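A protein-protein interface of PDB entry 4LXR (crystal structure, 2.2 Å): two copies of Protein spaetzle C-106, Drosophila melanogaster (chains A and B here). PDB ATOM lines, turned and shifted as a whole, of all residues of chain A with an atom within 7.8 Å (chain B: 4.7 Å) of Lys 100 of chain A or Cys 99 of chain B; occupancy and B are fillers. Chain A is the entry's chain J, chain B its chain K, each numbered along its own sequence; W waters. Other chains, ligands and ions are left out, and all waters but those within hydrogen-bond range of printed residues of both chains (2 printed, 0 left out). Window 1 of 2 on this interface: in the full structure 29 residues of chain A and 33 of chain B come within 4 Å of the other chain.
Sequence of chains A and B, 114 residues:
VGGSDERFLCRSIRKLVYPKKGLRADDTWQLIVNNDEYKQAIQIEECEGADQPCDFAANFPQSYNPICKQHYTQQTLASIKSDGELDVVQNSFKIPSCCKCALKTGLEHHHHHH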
ATOM      1  N   PHE A   8     -25.511  11.484  -3.226  1.00  0.00           N
ATOM      2  CA  PHE A   8     -25.689  10.144  -3.780  1.00  0.00           C
ATOM      3  C   PHE A   8     -26.078   9.190  -2.665  1.00  0.00           C
ATOM      4  O   PHE A   8     -25.952   9.522  -1.472  1.00  0.00           O
ATOM      5  CB  PHE A   8     -24.423   9.675  -4.491  1.00  0.00           C
ATOM      6  CG  PHE A   8     -23.941  10.643  -5.514  1.00  0.00           C
ATOM      7  CD1 PHE A   8     -24.505  10.665  -6.776  1.00  0.00           C
ATOM      8  CD2 PHE A   8     -22.960  11.562  -5.203  1.00  0.00           C
ATOM      9  CE1 PHE A   8     -24.081  11.567  -7.717  1.00  0.00           C
ATOM     10  CE2 PHE A   8     -22.532  12.476  -6.141  1.00  0.00           C
ATOM     11  CZ  PHE A   8     -23.095  12.481  -7.398  1.00  0.00           C
ATOM     12  N   LEU A   9     -26.530   8.007  -3.056  1.00  0.00           N
ATOM     13  CA  LEU A   9     -27.176   7.093  -2.123  1.00  0.00           C
ATOM     14  C   LEU A   9     -26.182   6.355  -1.248  1.00  0.00           C
ATOM     15  O   LEU A   9     -26.508   5.950  -0.134  1.00  0.00           O
ATOM     16  CB  LEU A   9     -28.028   6.095  -2.889  1.00  0.00           C
ATOM     17  CG  LEU A   9     -29.216   6.694  -3.626  1.00  0.00           C
ATOM     18  CD1 LEU A   9     -29.712   5.659  -4.553  1.00  0.00           C
ATOM     19  CD2 LEU A   9     -30.303   7.082  -2.628  1.00  0.00           C
ATOM     20  N   CYS A  10     -24.973   6.177  -1.757  1.00  0.00           N
ATOM     21  CA  CYS A  10     -23.943   5.505  -0.993  1.00  0.00           C
ATOM     22  C   CYS A  10     -22.745   6.433  -0.759  1.00  0.00           C
ATOM     23  O   CYS A  10     -22.072   6.849  -1.699  1.00  0.00           O
ATOM     24  CB  CYS A  10     -23.514   4.209  -1.685  1.00  0.00           C
ATOM     25  SG  CYS A  10     -24.774   2.896  -1.659  1.00  0.00           S
ATOM     26  N   ARG A  11     -22.503   6.763   0.500  1.00  0.00           N
ATOM     27  CA  ARG A  11     -21.332   7.551   0.866  1.00  0.00           C
ATOM     28  C   ARG A  11     -20.068   6.862   0.362  1.00  0.00           C
ATOM     29  O   ARG A  11     -19.966   5.635   0.362  1.00  0.00           O
ATOM     30  CB  ARG A  11     -21.276   7.771   2.385  1.00  0.00           C
ATOM     31  CG  ARG A  11     -22.420   8.636   2.884  1.00  0.00           C
ATOM     32  CD  ARG A  11     -22.710   8.494   4.375  1.00  0.00           C
ATOM     33  NE  ARG A  11     -24.020   9.067   4.697  1.00  0.00           N
ATOM     34  CZ  ARG A  11     -24.446   9.346   5.927  1.00  0.00           C
ATOM     35  NH1 ARG A  11     -23.664   9.113   6.974  1.00  0.00           N
ATOM     36  NH2 ARG A  11     -25.653   9.868   6.110  1.00  0.00           N
ATOM     37  N   SER A  12     -19.121   7.657  -0.106  1.00  0.00           N
ATOM     38  CA  SER A  12     -17.874   7.115  -0.597  1.00  0.00           C
ATOM     39  C   SER A  12     -16.746   8.100  -0.346  1.00  0.00           C
ATOM     40  O   SER A  12     -16.966   9.306  -0.242  1.00  0.00           O
ATOM     41  CB  SER A  12     -17.981   6.812  -2.086  1.00  0.00           C
ATOM     42  OG  SER A  12     -18.280   7.987  -2.814  1.00  0.00           O
ATOM     43  N   GLU A  45     -12.601   5.966  -6.017  1.00  0.00           N
ATOM     44  CA  GLU A  45     -13.746   6.189  -5.156  1.00  0.00           C
ATOM     45  C   GLU A  45     -14.086   4.862  -4.475  1.00  0.00           C
ATOM     46  O   GLU A  45     -14.367   3.864  -5.145  1.00  0.00           O
ATOM     47  CB  GLU A  45     -14.936   6.726  -5.963  1.00  0.00           C
ATOM     48  CG  GLU A  45     -16.226   6.898  -5.172  1.00  0.00           C
ATOM     49  CD  GLU A  45     -17.393   7.396  -6.028  1.00  0.00           C
ATOM     50  OE1 GLU A  45     -17.248   8.471  -6.656  1.00  0.00           O
ATOM     51  OE2 GLU A  45     -18.456   6.711  -6.070  1.00  0.00           O
ATOM     52  N   GLU A  46     -14.037   4.851  -3.145  1.00  0.00           N
ATOM     53  CA  GLU A  46     -14.276   3.643  -2.359  1.00  0.00           C
ATOM     54  C   GLU A  46     -15.497   3.792  -1.468  1.00  0.00           C
ATOM     55  O   GLU A  46     -15.676   4.827  -0.828  1.00  0.00           O
ATOM     56  CB  GLU A  46     -13.072   3.339  -1.462  1.00  0.00           C
ATOM     57  CG  GLU A  46     -11.925   2.609  -2.132  1.00  0.00           C
ATOM     58  CD  GLU A  46     -10.808   2.292  -1.154  1.00  0.00           C
ATOM     59  OE1 GLU A  46     -10.394   3.206  -0.407  1.00  0.00           O
ATOM     60  OE2 GLU A  46     -10.361   1.128  -1.118  1.00  0.00           O
ATOM     61  N   CYS A  47     -16.324   2.752  -1.408  1.00  0.00           N
ATOM     62  CA  CYS A  47     -17.480   2.766  -0.514  1.00  0.00           C
ATOM     63  C   CYS A  47     -17.048   2.944   0.942  1.00  0.00           C
ATOM     64  O   CYS A  47     -16.174   2.229   1.437  1.00  0.00           O
ATOM     65  CB  CYS A  47     -18.275   1.469  -0.641  1.00  0.00           C
ATOM     66  SG  CYS A  47     -19.157   1.298  -2.197  1.00  0.00           S
ATOM     67  N   GLY A  49     -19.223   2.328   3.122  1.00  0.00           N
ATOM     68  CA  GLY A  49     -20.017   1.251   3.696  1.00  0.00           C
ATOM     69  C   GLY A  49     -20.465   0.192   2.696  1.00  0.00           C
ATOM     70  O   GLY A  49     -21.667  -0.039   2.529  1.00  0.00           O
ATOM     71  N   ALA A  50     -19.502  -0.452   2.041  1.00  0.00           N
ATOM     72  CA  ALA A  50     -19.778  -1.548   1.114  1.00  0.00           C
ATOM     73  C   ALA A  50     -20.507  -2.685   1.815  1.00  0.00           C
ATOM     74  O   ALA A  50     -20.173  -3.029   2.948  1.00  0.00           O
ATOM     75  CB  ALA A  50     -18.480  -2.063   0.480  1.00  0.00           C
ATOM     76  N   ASP A  51     -21.512  -3.242   1.134  1.00  0.00           N
ATOM     77  CA  ASP A  51     -22.299  -4.378   1.632  1.00  0.00           C
ATOM     78  C   ASP A  51     -23.225  -4.009   2.782  1.00  0.00           C
ATOM     79  O   ASP A  51     -23.838  -4.877   3.387  1.00  0.00           O
ATOM     80  CB  ASP A  51     -21.410  -5.562   2.043  1.00  0.00           C
ATOM     81  CG  ASP A  51     -20.554  -6.077   0.903  1.00  0.00           C
ATOM     82  OD1 ASP A  51     -20.933  -5.891  -0.277  1.00  0.00           O
ATOM     83  OD2 ASP A  51     -19.501  -6.676   1.191  1.00  0.00           O
ATOM     84  N   GLN A  52     -23.314  -2.725   3.098  1.00  0.00           N
ATOM     85  CA  GLN A  52     -24.283  -2.273   4.080  1.00  0.00           C
ATOM     86  C   GLN A  52     -25.378  -1.534   3.342  1.00  0.00           C
ATOM     87  O   GLN A  52     -25.195  -1.161   2.184  1.00  0.00           O
ATOM     88  CB  GLN A  52     -23.617  -1.359   5.112  1.00  0.00           C
ATOM     89  CG  GLN A  52     -22.454  -2.002   5.822  1.00  0.00           C
ATOM     90  CD  GLN A  52     -22.849  -3.245   6.590  1.00  0.00           C
ATOM     91  OE1 GLN A  52     -22.089  -4.212   6.647  1.00  0.00           O
ATOM     92  NE2 GLN A  52     -24.025  -3.219   7.205  1.00  0.00           N
ATOM     93  N   CYS A  54     -27.857   1.145   1.684  1.00  0.00           N
ATOM     94  CA  CYS A  54     -27.744   2.504   1.143  1.00  0.00           C
ATOM     95  C   CYS A  54     -28.447   3.471   2.083  1.00  0.00           C
ATOM     96  O   CYS A  54     -29.300   3.048   2.867  1.00  0.00           O
ATOM     97  CB  CYS A  54     -28.426   2.581  -0.229  1.00  0.00           C
ATOM     98  SG  CYS A  54     -27.909   1.305  -1.402  1.00  0.00           S
ATOM     99  N   PRO A  66     -31.717  -2.533  -0.817  1.00  0.00           N
ATOM    100  CA  PRO A  66     -30.719  -1.526  -1.211  1.00  0.00           C
ATOM    101  C   PRO A  66     -29.417  -1.718  -0.455  1.00  0.00           C
ATOM    102  O   PRO A  66     -29.401  -1.594   0.765  1.00  0.00           O
ATOM    103  CB  PRO A  66     -31.360  -0.195  -0.786  1.00  0.00           C
ATOM    104  CG  PRO A  66     -32.795  -0.537  -0.408  1.00  0.00           C
ATOM    105  CD  PRO A  66     -32.734  -1.952   0.071  1.00  0.00           C
ATOM    106  N   ILE A  67     -28.351  -2.038  -1.179  1.00  0.00           N
ATOM    107  CA  ILE A  67     -27.058  -2.384  -0.584  1.00  0.00           C
ATOM    108  C   ILE A  67     -25.981  -1.663  -1.384  1.00  0.00           C
ATOM    109  O   ILE A  67     -26.009  -1.684  -2.621  1.00  0.00           O
ATOM    110  CB  ILE A  67     -26.810  -3.904  -0.661  1.00  0.00           C
ATOM    111  CG1 ILE A  67     -27.727  -4.652   0.312  1.00  0.00           C
ATOM    112  CG2 ILE A  67     -25.345  -4.235  -0.362  1.00  0.00           C
ATOM    113  CD1 ILE A  67     -27.435  -4.347   1.801  1.00  0.00           C
ATOM    114  N   CYS A  68     -25.043  -1.015  -0.695  1.00  0.00           N
ATOM    115  CA  CYS A  68     -23.995  -0.244  -1.372  1.00  0.00           C
ATOM    116  C   CYS A  68     -22.979  -1.220  -1.945  1.00  0.00           C
ATOM    117  O   CYS A  68     -22.575  -2.154  -1.270  1.00  0.00           O
ATOM    118  CB  CYS A  68     -23.301   0.733  -0.402  1.00  0.00           C
ATOM    119  SG  CYS A  68     -24.348   2.113   0.163  1.00  0.00           S
ATOM    120  N   LYS A  69     -22.575  -1.019  -3.192  1.00  0.00           N
ATOM    121  CA  LYS A  69     -21.634  -1.940  -3.808  1.00  0.00           C
ATOM    122  C   LYS A  69     -20.437  -1.201  -4.348  1.00  0.00           C
ATOM    123  O   LYS A  69     -20.573  -0.136  -4.952  1.00  0.00           O
ATOM    124  CB  LYS A  69     -22.289  -2.722  -4.941  1.00  0.00           C
ATOM    125  CG  LYS A  69     -23.563  -3.456  -4.528  1.00  0.00           C
ATOM    126  CD  LYS A  69     -23.365  -4.967  -4.448  1.00  0.00           C
ATOM    127  CE  LYS A  69     -22.582  -5.378  -3.216  1.00  0.00           C
ATOM    128  NZ  LYS A  69     -22.541  -6.857  -3.071  1.00  0.00           N
ATOM    129  N   GLN A  70     -19.267  -1.788  -4.128  1.00  0.00           N
ATOM    130  CA  GLN A  70     -18.032  -1.302  -4.714  1.00  0.00           C
ATOM    131  C   GLN A  70     -17.902  -1.867  -6.120  1.00  0.00           C
ATOM    132  O   GLN A  70     -17.996  -3.075  -6.330  1.00  0.00           O
ATOM    133  CB  GLN A  70     -16.840  -1.739  -3.861  1.00  0.00           C
ATOM    134  CG  GLN A  70     -15.474  -1.227  -4.365  1.00  0.00           C
ATOM    135  CD  GLN A  70     -15.353   0.273  -4.243  1.00  0.00           C
ATOM    136  OE1 GLN A  70     -15.285   0.809  -3.138  1.00  0.00           O
ATOM    137  NE2 GLN A  70     -15.366   0.966  -5.381  1.00  0.00           N
ATOM    138  N   HIS A  71     -17.715  -0.978  -7.086  1.00  0.00           N
ATOM    139  CA  HIS A  71     -17.463  -1.371  -8.466  1.00  0.00           C
ATOM    140  C   HIS A  71     -16.019  -1.076  -8.811  1.00  0.00           C
ATOM    141  O   HIS A  71     -15.367  -0.234  -8.172  1.00  0.00           O
ATOM    142  CB  HIS A  71     -18.381  -0.617  -9.435  1.00  0.00           C
ATOM    143  CG  HIS A  71     -19.812  -1.045  -9.368  1.00  0.00           C
ATOM    144  ND1 HIS A  71     -20.375  -1.910 -10.282  1.00  0.00           N
ATOM    145  CD2 HIS A  71     -20.798  -0.725  -8.497  1.00  0.00           C
ATOM    146  CE1 HIS A  71     -21.644  -2.106  -9.975  1.00  0.00           C
ATOM    147  NE2 HIS A  71     -21.927  -1.397  -8.900  1.00  0.00           N
ATOM    148  N   SER A  97     -13.588   2.131  -8.617  1.00  0.00           N
ATOM    149  CA  SER A  97     -13.946   3.194  -9.539  1.00  0.00           C
ATOM    150  C   SER A  97     -15.170   3.964  -9.076  1.00  0.00           C
ATOM    151  O   SER A  97     -15.339   5.150  -9.389  1.00  0.00           O
ATOM    152  CB  SER A  97     -14.241   2.584 -10.908  1.00  0.00           C
ATOM    153  OG  SER A  97     -15.394   1.759 -10.840  1.00  0.00           O
ATOM    154  N   CYS A  98     -16.031   3.280  -8.333  1.00  0.00           N
ATOM    155  CA  CYS A  98     -17.348   3.807  -8.087  1.00  0.00           C
ATOM    156  C   CYS A  98     -18.043   3.052  -6.963  1.00  0.00           C
ATOM    157  O   CYS A  98     -17.960   1.830  -6.875  1.00  0.00           O
ATOM    158  CB  CYS A  98     -18.137   3.673  -9.390  1.00  0.00           C
ATOM    159  SG  CYS A  98     -19.836   4.203  -9.345  1.00  0.00           S
ATOM    160  N   CYS A  99     -18.729   3.783  -6.094  1.00  0.00           N
ATOM    161  CA  CYS A  99     -19.582   3.153  -5.094  1.00  0.00           C
ATOM    162  C   CYS A  99     -21.046   3.421  -5.437  1.00  0.00           C
ATOM    163  O   CYS A  99     -21.463   4.575  -5.576  1.00  0.00           O
ATOM    164  CB  CYS A  99     -19.266   3.679  -3.699  1.00  0.00           C
ATOM    165  SG  CYS A  99     -20.292   2.979  -2.389  1.00  0.00           S
ATOM    166  N   LYS A 100     -21.830   2.358  -5.561  1.00  0.00           N
ATOM    167  CA  LYS A 100     -23.171   2.484  -6.134  1.00  0.00           C
ATOM    168  C   LYS A 100     -24.194   1.658  -5.370  1.00  0.00           C
ATOM    169  O   LYS A 100     -23.887   0.565  -4.893  1.00  0.00           O
ATOM    170  CB  LYS A 100     -23.137   2.043  -7.599  1.00  0.00           C
ATOM    171  CG  LYS A 100     -23.942   2.919  -8.534  1.00  0.00           C
ATOM    172  CD  LYS A 100     -23.465   2.776  -9.969  1.00  0.00           C
ATOM    173  CE  LYS A 100     -23.683   1.374 -10.496  1.00  0.00           C
ATOM    174  NZ  LYS A 100     -23.545   1.324 -11.977  1.00  0.00           N
ATOM    175  N   CYS A 101     -25.412   2.184  -5.256  1.00  0.00           N
ATOM    176  CA  CYS A 101     -26.505   1.470  -4.592  1.00  0.00           C
ATOM    177  C   CYS A 101     -27.181   0.448  -5.509  1.00  0.00           C
ATOM    178  O   CYS A 101     -27.803   0.805  -6.495  1.00  0.00           O
ATOM    179  CB  CYS A 101     -27.546   2.455  -4.062  1.00  0.00           C
ATOM    180  SG  CYS A 101     -28.881   1.676  -3.150  1.00  0.00           S
ATOM    181  N   ALA A 102     -27.041  -0.825  -5.165  1.00  0.00           N
ATOM    182  CA  ALA A 102     -27.651  -1.909  -5.921  1.00  0.00           C
ATOM    183  C   ALA A 102     -28.948  -2.301  -5.245  1.00  0.00           C
ATOM    184  O   ALA A 102     -28.982  -2.474  -4.032  1.00  0.00           O
ATOM    185  CB  ALA A 102     -26.701  -3.125  -5.984  1.00  0.00           C
ATOM    186  N   LEU A 103     -30.018  -2.428  -6.019  1.00  0.00           N
ATOM    187  CA  LEU A 103     -31.274  -2.900  -5.457  1.00  0.00           C
ATOM    188  C   LEU A 103     -31.325  -4.389  -5.717  1.00  0.00           C
ATOM    189  O   LEU A 103     -31.590  -4.815  -6.836  1.00  0.00           O
ATOM    190  CB  LEU A 103     -32.490  -2.191  -6.090  1.00  0.00           C
ATOM    191  CG  LEU A 103     -32.532  -0.653  -6.018  1.00  0.00           C
ATOM    192  CD1 LEU A 103     -33.890  -0.085  -6.450  1.00  0.00           C
ATOM    193  CD2 LEU A 103     -32.187  -0.131  -4.632  1.00  0.00           C
ATOM    194  N   PHE B   8     -30.093  -1.141 -10.746  1.00  0.00           N
ATOM    195  CA  PHE B   8     -29.495   0.134 -10.449  1.00  0.00           C
ATOM    196  C   PHE B   8     -30.414   1.263 -10.878  1.00  0.00           C
ATOM    197  O   PHE B   8     -31.221   1.105 -11.793  1.00  0.00           O
ATOM    198  CB  PHE B   8     -28.150   0.229 -11.157  1.00  0.00           C
ATOM    199  CG  PHE B   8     -27.153  -0.754 -10.649  1.00  0.00           C
ATOM    200  CD1 PHE B   8     -26.489  -0.519  -9.451  1.00  0.00           C
ATOM    201  CD2 PHE B   8     -26.899  -1.928 -11.340  1.00  0.00           C
ATOM    202  CE1 PHE B   8     -25.568  -1.425  -8.967  1.00  0.00           C
ATOM    203  CE2 PHE B   8     -25.983  -2.842 -10.857  1.00  0.00           C
ATOM    204  CZ  PHE B   8     -25.318  -2.594  -9.671  1.00  0.00           C
ATOM    205  N   CYS B  10     -29.711   3.925 -12.411  1.00  0.00           N
ATOM    206  CA  CYS B  10     -29.376   4.487 -13.709  1.00  0.00           C
ATOM    207  C   CYS B  10     -28.910   3.443 -14.695  1.00  0.00           C
ATOM    208  O   CYS B  10     -28.153   2.539 -14.356  1.00  0.00           O
ATOM    209  CB  CYS B  10     -28.320   5.578 -13.550  1.00  0.00           C
ATOM    210  SG  CYS B  10     -28.914   6.978 -12.568  1.00  0.00           S
ATOM    211  N   ARG B  11     -29.366   3.581 -15.931  1.00  0.00           N
ATOM    212  CA  ARG B  11     -28.896   2.723 -17.006  1.00  0.00           C
ATOM    213  C   ARG B  11     -27.510   3.167 -17.467  1.00  0.00           C
ATOM    214  O   ARG B  11     -27.275   4.357 -17.711  1.00  0.00           O
ATOM    215  CB  ARG B  11     -29.849   2.789 -18.182  1.00  0.00           C
ATOM    216  CG  ARG B  11     -31.238   2.254 -17.900  1.00  0.00           C
ATOM    217  CD  ARG B  11     -31.968   2.133 -19.207  1.00  0.00           C
ATOM    218  NE  ARG B  11     -33.319   1.628 -19.037  1.00  0.00           N
ATOM    219  CZ  ARG B  11     -34.034   1.095 -20.019  1.00  0.00           C
ATOM    220  NH1 ARG B  11     -35.265   0.670 -19.785  1.00  0.00           N
ATOM    221  NH2 ARG B  11     -33.512   0.984 -21.234  1.00  0.00           N
ATOM    222  N   SER B  12     -26.610   2.197 -17.601  1.00  0.00           N
ATOM    223  CA  SER B  12     -25.270   2.453 -18.095  1.00  0.00           C
ATOM    224  C   SER B  12     -24.776   1.321 -18.993  1.00  0.00           C
ATOM    225  O   SER B  12     -25.220   0.171 -18.874  1.00  0.00           O
ATOM    226  CB  SER B  12     -24.311   2.608 -16.924  1.00  0.00           C
ATOM    227  OG  SER B  12     -24.205   1.379 -16.225  1.00  0.00           O
ATOM    228  N   GLU B  45     -17.561   3.214 -18.007  1.00  0.00           N
ATOM    229  CA  GLU B  45     -19.003   3.126 -17.836  1.00  0.00           C
ATOM    230  C   GLU B  45     -19.637   4.474 -18.123  1.00  0.00           C
ATOM    231  O   GLU B  45     -19.261   5.479 -17.515  1.00  0.00           O
ATOM    232  CB  GLU B  45     -19.367   2.660 -16.427  1.00  0.00           C
ATOM    233  CG  GLU B  45     -20.875   2.463 -16.226  1.00  0.00           C
ATOM    234  CD  GLU B  45     -21.201   1.811 -14.900  1.00  0.00           C
ATOM    235  OE1 GLU B  45     -21.953   2.410 -14.091  1.00  0.00           O
ATOM    236  OE2 GLU B  45     -20.687   0.694 -14.673  1.00  0.00           O
ATOM    237  N   GLU B  46     -20.585   4.496 -19.056  1.00  0.00           N
ATOM    238  CA  GLU B  46     -21.257   5.736 -19.448  1.00  0.00           C
ATOM    239  C   GLU B  46     -22.744   5.642 -19.210  1.00  0.00           C
ATOM    240  O   GLU B  46     -23.325   4.584 -19.412  1.00  0.00           O
ATOM    241  CB  GLU B  46     -21.041   6.033 -20.930  1.00  0.00           C
ATOM    242  CG  GLU B  46     -19.664   6.529 -21.284  1.00  0.00           C
ATOM    243  CD  GLU B  46     -19.548   6.888 -22.749  1.00  0.00           C
ATOM    244  OE1 GLU B  46     -19.979   6.071 -23.591  1.00  0.00           O
ATOM    245  OE2 GLU B  46     -19.033   7.989 -23.055  1.00  0.00           O
ATOM    246  N   CYS B  47     -23.357   6.749 -18.793  1.00  0.00           N
ATOM    247  CA  CYS B  47     -24.804   6.808 -18.667  1.00  0.00           C
ATOM    248  C   CYS B  47     -25.440   6.520 -20.033  1.00  0.00           C
ATOM    249  O   CYS B  47     -24.984   7.040 -21.052  1.00  0.00           O
ATOM    250  CB  CYS B  47     -25.258   8.176 -18.147  1.00  0.00           C
ATOM    251  SG  CYS B  47     -24.704   8.587 -16.457  1.00  0.00           S
ATOM    252  N   CYS B  68     -29.876  11.131 -13.407  1.00  0.00           N
ATOM    253  CA  CYS B  68     -28.702  10.311 -13.627  1.00  0.00           C
ATOM    254  C   CYS B  68     -27.538  11.198 -14.072  1.00  0.00           C
ATOM    255  O   CYS B  68     -27.672  12.014 -14.985  1.00  0.00           O
ATOM    256  CB  CYS B  68     -29.012   9.210 -14.642  1.00  0.00           C
ATOM    257  SG  CYS B  68     -30.112   7.909 -13.955  1.00  0.00           S
ATOM    258  N   LYS B  69     -26.401  11.052 -13.401  1.00  0.00           N
ATOM    259  CA  LYS B  69     -25.222  11.850 -13.703  1.00  0.00           C
ATOM    260  C   LYS B  69     -24.022  10.987 -14.050  1.00  0.00           C
ATOM    261  O   LYS B  69     -23.819   9.914 -13.475  1.00  0.00           O
ATOM    262  CB  LYS B  69     -24.864  12.746 -12.519  1.00  0.00           C
ATOM    263  CG  LYS B  69     -25.962  13.716 -12.152  1.00  0.00           C
ATOM    264  CD  LYS B  69     -26.273  14.645 -13.310  1.00  0.00           C
ATOM    265  CE  LYS B  69     -26.038  16.079 -12.910  1.00  0.00           C
ATOM    266  NZ  LYS B  69     -26.723  16.348 -11.614  1.00  0.00           N
ATOM    267  N   CYS B  98     -18.619   5.586 -13.968  1.00  0.00           N
ATOM    268  CA  CYS B  98     -19.938   5.049 -13.629  1.00  0.00           C
ATOM    269  C   CYS B  98     -21.034   6.107 -13.742  1.00  0.00           C
ATOM    270  O   CYS B  98     -20.749   7.300 -13.882  1.00  0.00           O
ATOM    271  CB  CYS B  98     -19.968   4.419 -12.225  1.00  0.00           C
ATOM    272  SG  CYS B  98     -19.800   5.566 -10.858  1.00  0.00           S
ATOM    273  N   CYS B  99     -22.281   5.645 -13.662  1.00  0.00           N
ATOM    274  CA  CYS B  99     -23.460   6.492 -13.763  1.00  0.00           C
ATOM    275  C   CYS B  99     -24.234   6.385 -12.463  1.00  0.00           C
ATOM    276  O   CYS B  99     -24.580   5.294 -12.022  1.00  0.00           O
ATOM    277  CB  CYS B  99     -24.341   6.011 -14.917  1.00  0.00           C
ATOM    278  SG  CYS B  99     -25.681   7.125 -15.396  1.00  0.00           S
ATOM    279  N   LYS B 100     -24.502   7.509 -11.821  1.00  0.00           N
ATOM    280  CA  LYS B 100     -25.143   7.440 -10.511  1.00  0.00           C
ATOM    281  C   LYS B 100     -26.304   8.399 -10.425  1.00  0.00           C
ATOM    282  O   LYS B 100     -26.330   9.422 -11.111  1.00  0.00           O
ATOM    283  CB  LYS B 100     -24.140   7.748  -9.390  1.00  0.00           C
ATOM    284  CG  LYS B 100     -22.889   6.887  -9.432  1.00  0.00           C
ATOM    285  CD  LYS B 100     -22.188   6.811  -8.070  1.00  0.00           C
ATOM    286  CE  LYS B 100     -21.370   8.046  -7.769  1.00  0.00           C
ATOM    287  NZ  LYS B 100     -20.786   7.941  -6.404  1.00  0.00           N
ATOM    288  N   CYS B 101     -27.243   8.079  -9.549  1.00  0.00           N
ATOM    289  CA  CYS B 101     -28.417   8.906  -9.377  1.00  0.00           C
ATOM    290  C   CYS B 101     -28.124   9.979  -8.347  1.00  0.00           C
ATOM    291  O   CYS B 101     -27.781   9.676  -7.209  1.00  0.00           O
ATOM    292  CB  CYS B 101     -29.616   8.062  -8.942  1.00  0.00           C
ATOM    293  SG  CYS B 101     -31.103   9.034  -8.683  1.00  0.00           S
HETATM  294  O   HOH W   1     -21.040   8.194  -3.781  1.00  0.00           O
HETATM  295  O   HOH W   2     -26.761   7.870  -5.965  1.00  0.00           O
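OE2 of Glu 45 of chain A lies within salt-bridge range of NZ of Lys 100 of chain B (2.7 Å).
SG of Cys 98 of chain A forms a disulfide with SG of Cys 98 of chain B.
The side-chain amino group (NZ) of Lys 100 of chain A is in salt-bridge range of the side-chain carboxylate (OE1) of Glu 45 of chain B (2.9 Å).
CB of Lys 100 of chain B touches CD1 of Phe 8 of chain A (3.9 Å).
Phe 8 of chain A touches Cys 101 of chain B.
His 71 of chain A touches Phe 8 of chain B (NE2 to CE1, 3.6 Å).
Lys 100 of chain B touches Cys 98 of chain A.
Cys 99 of chain A touches Lys 100 of chain B.
CE of Lys 100 of chain A touches CD1 of Phe 8 of chain B, at 3.5 Å.
Lys 100 of chain A touches Cys 99 of chain B (CD to O, 3.4 Å).
O of Cys 101 of chain A touches CD1 of Phe 8 of chain B, 3.5 Å away.
Ala 102 of chain A touches Phe 8 of chain B (CB to CE1, 3.6 Å).
The backbone NH (N) of Cys 99 of chain A lies within hydrogen-bond range of the side-chain carboxylate (OE2) of Glu 45 of chain A (2.9 Å).
The backbone carbonyl oxygen (O) of Ile 67 of chain A is in hydrogen-bond range of the backbone NH (N) of Ala 102 of chain A (2.9 Å).
N of Lys 69 of chain A sits at hydrogen-bond distance from O of Lys 100 of chain A (2.7 Å).
NE2 of Gln 70 of chain A lies within hydrogen-bond range of O of Cys 98 of chain A.
SG of Cys 99 of chain B forms a disulfide with SG of Cys 47 of chain B (2.1 Å).
SG of Cys 68 of chain B is disulfide-bonded to SG of Cys 10 of chain B (2.1 Å).
Phe 8 of chain A touches Lys 100 of chain B, and with the chains exchanged Lys 100 of chain A touches Phe 8 of chain B.
Phe 8 of chain A touches Cys 101 of chain B, and with the chains exchanged Cys 101 of chain A touches Phe 8 of chain B.
Glu 45 of chain A touches Lys 100 of chain B, and with the chains exchanged Lys 100 of chain A touches Glu 45 of chain B.
Cys 99 of chain A touches Lys 100 of chain B, and with the chains exchanged Lys 100 of chain A touches Cys 99 of chain B.
Of the printed residues of chain B, Phe 8 of chain A touches Lys 100 and Cys 101.
Printed residues of chain B within 4 Å of Cys 98 of chain A: Cys 98 (2.0 Å) and Lys 100 (3.7 Å).
Lys 100 of chain A touches just these residues of chain B: Phe 8 (3.5 Å), Glu 45 (2.9 Å) and Cys 99 (3.4 Å).
Of the printed residues of chain B, Cys 101 of chain A touches Phe 8 (3.5 Å).
Cys 68 of chain B touches none of the printed residues of chain A.
Cys 99 of chain B touches just one residue of chain A: Lys 100.
Printed residues of chain A that touch a printed residue of chain B: Phe 8, Glu 45, His 71, Cys 98, Cys 99, Lys 100, Cys 101 and Ala 102.
Of the 13 printed residues of chain B, 6 touch a printed residue of chain A.
Hydrophobic or aromatic side chains of chain B within 4 Å of the printed part of chain A: Phe 8.
Among the printed residues, 12 pairs touch across the chains.
Water W2 bridges O of Cys 101 of chain B (2.4 Å) and N of Leu 9 of chain A (2.9 Å).
Water W1 lies within hydrogen-bond range of the side-chain amino group of Lys 100 of chain B, the backbone carbonyl oxygen of Cys 10 of chain A and the side-chain hydroxyl of Ser 12 of chain A.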
